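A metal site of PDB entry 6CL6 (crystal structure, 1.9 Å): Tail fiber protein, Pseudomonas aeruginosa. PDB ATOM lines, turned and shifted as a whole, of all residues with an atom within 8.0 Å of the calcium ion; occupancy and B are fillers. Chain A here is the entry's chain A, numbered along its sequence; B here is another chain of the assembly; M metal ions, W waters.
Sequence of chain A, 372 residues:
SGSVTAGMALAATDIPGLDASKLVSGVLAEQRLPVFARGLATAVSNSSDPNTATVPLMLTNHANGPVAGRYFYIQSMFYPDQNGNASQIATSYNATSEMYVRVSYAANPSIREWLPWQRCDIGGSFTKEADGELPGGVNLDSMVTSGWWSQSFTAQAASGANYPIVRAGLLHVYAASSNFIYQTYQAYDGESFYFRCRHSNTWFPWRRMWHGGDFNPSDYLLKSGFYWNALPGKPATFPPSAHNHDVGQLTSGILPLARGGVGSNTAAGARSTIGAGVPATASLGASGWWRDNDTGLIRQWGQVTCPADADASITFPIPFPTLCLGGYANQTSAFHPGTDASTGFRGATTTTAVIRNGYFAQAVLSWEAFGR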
ATOM      1  N   ALA A 308      18.691  18.533  21.267  1.00  0.00           N
ATOM      2  CA  ALA A 308      19.044  19.357  20.123  1.00  0.00           C
ATOM      3  C   ALA A 308      17.862  20.259  19.740  1.00  0.00           C
ATOM      4  O   ALA A 308      16.726  19.794  19.659  1.00  0.00           O
ATOM      5  CB  ALA A 308      19.425  18.467  18.943  1.00  0.00           C
ATOM      6  N   ASP A 309      18.126  21.538  19.520  1.00  0.00           N
ATOM      7  CA  ASP A 309      17.131  22.452  18.944  1.00  0.00           C
ATOM      8  C   ASP A 309      15.794  22.385  19.676  1.00  0.00           C
ATOM      9  O   ASP A 309      14.737  22.364  19.050  1.00  0.00           O
ATOM     10  CB  ASP A 309      16.919  22.126  17.432  1.00  0.00           C
ATOM     11  CG  ASP A 309      18.131  22.440  16.580  1.00  0.00           C
ATOM     12  OD1 ASP A 309      18.860  23.419  16.860  1.00  0.00           O
ATOM     13  OD2 ASP A 309      18.342  21.696  15.578  1.00  0.00           O
ATOM     14  N   ALA A 310      15.820  22.367  21.008  1.00  0.00           N
ATOM     15  CA  ALA A 310      14.587  22.070  21.759  1.00  0.00           C
ATOM     16  C   ALA A 310      14.724  22.532  23.200  1.00  0.00           C
ATOM     17  O   ALA A 310      15.787  22.987  23.622  1.00  0.00           O
ATOM     18  CB  ALA A 310      14.257  20.577  21.710  1.00  0.00           C
ATOM     19  N   THR A 339      27.519  26.615  13.342  1.00  0.00           N
ATOM     20  CA  THR A 339      26.076  26.642  13.446  1.00  0.00           C
ATOM     21  C   THR A 339      25.660  27.531  14.623  1.00  0.00           C
ATOM     22  O   THR A 339      26.489  27.991  15.386  1.00  0.00           O
ATOM     23  CB  THR A 339      25.522  25.212  13.585  1.00  0.00           C
ATOM     24  OG1 THR A 339      24.102  25.228  13.432  1.00  0.00           O
ATOM     25  CG2 THR A 339      25.852  24.630  14.953  1.00  0.00           C
ATOM     26  N   ASP A 340      24.341  27.761  14.743  1.00  0.00           N
ATOM     27  CA  ASP A 340      23.829  28.530  15.861  1.00  0.00           C
ATOM     28  C   ASP A 340      23.926  27.727  17.176  1.00  0.00           C
ATOM     29  O   ASP A 340      23.749  26.492  17.203  1.00  0.00           O
ATOM     30  CB  ASP A 340      22.383  28.958  15.644  1.00  0.00           C
ATOM     31  CG  ASP A 340      21.764  29.622  16.898  1.00  0.00           C
ATOM     32  OD1 ASP A 340      22.022  30.831  17.119  1.00  0.00           O
ATOM     33  OD2 ASP A 340      21.029  28.944  17.672  1.00  0.00           O
ATOM     34  N   ALA A 341      24.221  28.418  18.250  1.00  0.00           N
ATOM     35  CA  ALA A 341      24.224  27.812  19.599  1.00  0.00           C
ATOM     36  C   ALA A 341      23.555  28.782  20.566  1.00  0.00           C
ATOM     37  O   ALA A 341      24.028  29.032  21.667  1.00  0.00           O
ATOM     38  CB  ALA A 341      25.626  27.439  20.036  1.00  0.00           C
ATOM     39  N   SER A 342      22.412  29.293  20.168  1.00  0.00           N
ATOM     40  CA  SER A 342      21.660  30.247  20.973  1.00  0.00           C
ATOM     41  C   SER A 342      21.056  29.565  22.194  1.00  0.00           C
ATOM     42  O   SER A 342      20.972  28.355  22.287  1.00  0.00           O
ATOM     43  CB  SER A 342      20.549  30.883  20.122  1.00  0.00           C
ATOM     44  OG  SER A 342      21.097  31.765  19.181  1.00  0.00           O
ATOM     45  N   ASN A 357      17.481  25.346  23.877  1.00  0.00           N
ATOM     46  CA  ASN A 357      18.801  25.077  23.307  1.00  0.00           C
ATOM     47  C   ASN A 357      18.732  25.170  21.790  1.00  0.00           C
ATOM     48  O   ASN A 357      18.165  24.302  21.127  1.00  0.00           O
ATOM     49  CB  ASN A 357      19.298  23.709  23.733  1.00  0.00           C
ATOM     50  CG  ASN A 357      20.554  23.294  23.032  1.00  0.00           C
ATOM     51  OD1 ASN A 357      21.408  24.121  22.741  1.00  0.00           O
ATOM     52  ND2 ASN A 357      20.664  22.008  22.729  1.00  0.00           N
ATOM     53  N   GLY A 358      19.325  26.233  21.241  1.00  0.00           N
ATOM     54  CA  GLY A 358      19.407  26.386  19.797  1.00  0.00           C
ATOM     55  C   GLY A 358      20.483  25.582  19.119  1.00  0.00           C
ATOM     56  O   GLY A 358      20.499  25.546  17.903  1.00  0.00           O
ATOM     57  N   TYR A 359      21.377  24.938  19.865  1.00  0.00           N
ATOM     58  CA  TYR A 359      22.452  24.151  19.267  1.00  0.00           C
ATOM     59  C   TYR A 359      21.909  22.819  18.768  1.00  0.00           C
ATOM     60  O   TYR A 359      21.039  22.223  19.428  1.00  0.00           O
ATOM     61  CB  TYR A 359      23.554  23.904  20.273  1.00  0.00           C
ATOM     62  CG  TYR A 359      24.768  23.176  19.704  1.00  0.00           C
ATOM     63  CD1 TYR A 359      25.422  23.663  18.600  1.00  0.00           C
ATOM     64  CD2 TYR A 359      25.293  22.042  20.325  1.00  0.00           C
ATOM     65  CE1 TYR A 359      26.540  22.999  18.075  1.00  0.00           C
ATOM     66  CE2 TYR A 359      26.375  21.403  19.851  1.00  0.00           C
ATOM     67  CZ  TYR A 359      27.011  21.881  18.706  1.00  0.00           C
ATOM     68  OH  TYR A 359      28.108  21.242  18.223  1.00  0.00           O
ATOM     69  N   PHE A 360      22.436  22.323  17.642  1.00  0.00           N
ATOM     70  CA  PHE A 360      21.867  21.155  16.965  1.00  0.00           C
ATOM     71  C   PHE A 360      22.369  19.835  17.513  1.00  0.00           C
ATOM     72  O   PHE A 360      22.591  18.878  16.756  1.00  0.00           O
ATOM     73  CB  PHE A 360      22.104  21.272  15.454  1.00  0.00           C
ATOM     74  CG  PHE A 360      23.543  21.239  14.983  1.00  0.00           C
ATOM     75  CD1 PHE A 360      24.607  21.006  15.824  1.00  0.00           C
ATOM     76  CD2 PHE A 360      23.808  21.431  13.621  1.00  0.00           C
ATOM     77  CE1 PHE A 360      25.917  20.939  15.349  1.00  0.00           C
ATOM     78  CE2 PHE A 360      25.126  21.367  13.125  1.00  0.00           C
ATOM     79  CZ  PHE A 360      26.177  21.121  13.979  1.00  0.00           C
ATOM     80  N   ALA A 361      22.567  19.756  18.831  1.00  0.00           N
ATOM     81  CA  ALA A 361      22.930  18.522  19.496  1.00  0.00           C
ATOM     82  C   ALA A 361      22.536  18.616  20.957  1.00  0.00           C
ATOM     83  O   ALA A 361      22.461  19.710  21.511  1.00  0.00           O
ATOM     84  CB  ALA A 361      24.421  18.199  19.381  1.00  0.00           C
ATOM     85  N   PHE B 335      12.263  30.783  20.067  1.00  0.00           N
ATOM     86  CA  PHE B 335      12.798  31.122  18.764  1.00  0.00           C
ATOM     87  C   PHE B 335      12.960  29.852  17.916  1.00  0.00           C
ATOM     88  O   PHE B 335      13.275  28.777  18.422  1.00  0.00           O
ATOM     89  CB  PHE B 335      14.139  31.837  18.887  1.00  0.00           C
ATOM     90  CG  PHE B 335      15.174  31.095  19.689  1.00  0.00           C
ATOM     91  CD1 PHE B 335      15.957  30.147  19.117  1.00  0.00           C
ATOM     92  CD2 PHE B 335      15.346  31.376  21.041  1.00  0.00           C
ATOM     93  CE1 PHE B 335      16.907  29.474  19.857  1.00  0.00           C
ATOM     94  CE2 PHE B 335      16.276  30.696  21.792  1.00  0.00           C
ATOM     95  CZ  PHE B 335      17.066  29.753  21.209  1.00  0.00           C
ATOM     96  N   HIS B 336      12.738  30.001  16.617  1.00  0.00           N
ATOM     97  CA  HIS B 336      12.912  28.895  15.709  1.00  0.00           C
ATOM     98  C   HIS B 336      14.348  28.407  15.796  1.00  0.00           C
ATOM     99  O   HIS B 336      15.268  29.215  15.571  1.00  0.00           O
ATOM    100  CB  HIS B 336      12.569  29.312  14.285  1.00  0.00           C
ATOM    101  CG  HIS B 336      12.458  28.161  13.338  1.00  0.00           C
ATOM    102  ND1 HIS B 336      13.557  27.612  12.712  1.00  0.00           N
ATOM    103  CD2 HIS B 336      11.393  27.428  12.947  1.00  0.00           C
ATOM    104  CE1 HIS B 336      13.160  26.613  11.940  1.00  0.00           C
ATOM    105  NE2 HIS B 336      11.850  26.480  12.076  1.00  0.00           N
ATOM    106  N   PRO B 337      14.602  27.144  16.153  1.00  0.00           N
ATOM    107  CA  PRO B 337      15.993  26.700  16.358  1.00  0.00           C
ATOM    108  C   PRO B 337      16.695  26.307  15.074  1.00  0.00           C
ATOM    109  O   PRO B 337      17.820  25.820  15.137  1.00  0.00           O
ATOM    110  CB  PRO B 337      15.832  25.494  17.282  1.00  0.00           C
ATOM    111  CG  PRO B 337      14.480  24.918  16.916  1.00  0.00           C
ATOM    112  CD  PRO B 337      13.629  26.065  16.391  1.00  0.00           C
ATOM    113  N   GLY B 338      16.069  26.489  13.930  1.00  0.00           N
ATOM    114  CA  GLY B 338      16.750  26.326  12.669  1.00  0.00           C
ATOM    115  C   GLY B 338      17.474  27.574  12.194  1.00  0.00           C
ATOM    116  O   GLY B 338      18.022  27.563  11.083  1.00  0.00           O
ATOM    117  N   THR B 339      17.500  28.651  12.986  1.00  0.00           N
ATOM    118  CA  THR B 339      18.149  29.895  12.588  1.00  0.00           C
ATOM    119  C   THR B 339      18.976  30.402  13.778  1.00  0.00           C
ATOM    120  O   THR B 339      19.018  29.779  14.842  1.00  0.00           O
ATOM    121  CB  THR B 339      17.131  30.933  12.109  1.00  0.00           C
ATOM    122  OG1 THR B 339      17.791  32.018  11.424  1.00  0.00           O
ATOM    123  CG2 THR B 339      16.339  31.475  13.275  1.00  0.00           C
ATOM    124  N   ASP B 340      19.662  31.527  13.578  1.00  0.00           N
ATOM    125  CA  ASP B 340      20.404  32.156  14.658  1.00  0.00           C
ATOM    126  C   ASP B 340      19.507  33.110  15.457  1.00  0.00           C
ATOM    127  O   ASP B 340      18.593  33.732  14.936  1.00  0.00           O
ATOM    128  CB  ASP B 340      21.631  32.913  14.115  1.00  0.00           C
ATOM    129  CG  ASP B 340      21.323  33.774  12.896  1.00  0.00           C
ATOM    130  OD1 ASP B 340      21.482  33.279  11.739  1.00  0.00           O
ATOM    131  OD2 ASP B 340      20.937  34.954  13.085  1.00  0.00           O
HETATM  132 CA    CA M   1      19.899  25.171  15.628  1.00  0.00          CA
HETATM  133  O   HOH W   1      22.283  24.747  15.580  1.00  0.00           O
HETATM  134  O   HOH W   2      19.854  23.261  14.046  1.00  0.00           O
HETATM  135  O   HOH W   3      19.565  27.545  16.323  1.00  0.00           O
HETATM  136  O   HOH W   4      20.251  26.227  13.520  1.00  0.00           O
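Water W1 lies within hydrogen-bond range of O of Asp 340 of chain A (2.8 Å), OG1 of Thr 339 of chain A (2.9 Å) and N of Phe 360 (3.2 Å). Water W3 lies within hydrogen-bond range of the side-chain carboxylate (OD2) of Asp 340 of chain A (2.4 Å) and the backbone carbonyl oxygen (O) of Thr 339 of chain B (2.7 Å).
Of the 18 residues printed, 3 come within 4 Å of the calcium ion. Along chain A the residues within 4 Å of the calcium ion span positions 309 to 358.
The backbone carbonyl oxygen of Tyr 359 is in hydrogen-bond range of the backbone NH of Asp 309. The backbone NH of Asp 309 sits close to the backbone carbonyl oxygen of Asn 357, 3.2 Å away. The backbone carbonyl oxygen of Ser 342 is in hydrogen-bond range of the backbone NH of Gly 358, at 2.9 Å.
The calcium ion is bound by the backbone carbonyl oxygen (O) of Pro 337 of chain B. OD1 of Asp 309 is bound to the calcium ion (2.4 Å). The calcium ion is bound by O of Gly 358, at 2.4 Å. Water W4 binds the calcium ion, at 2.4 Å. Water W1 is bound to the calcium ion, at 2.4 Å. The calcium ion is bound by water W2. Water W3 is bound to the calcium ion (2.5 Å). The calcium ion has seven donor atoms within binding distance.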
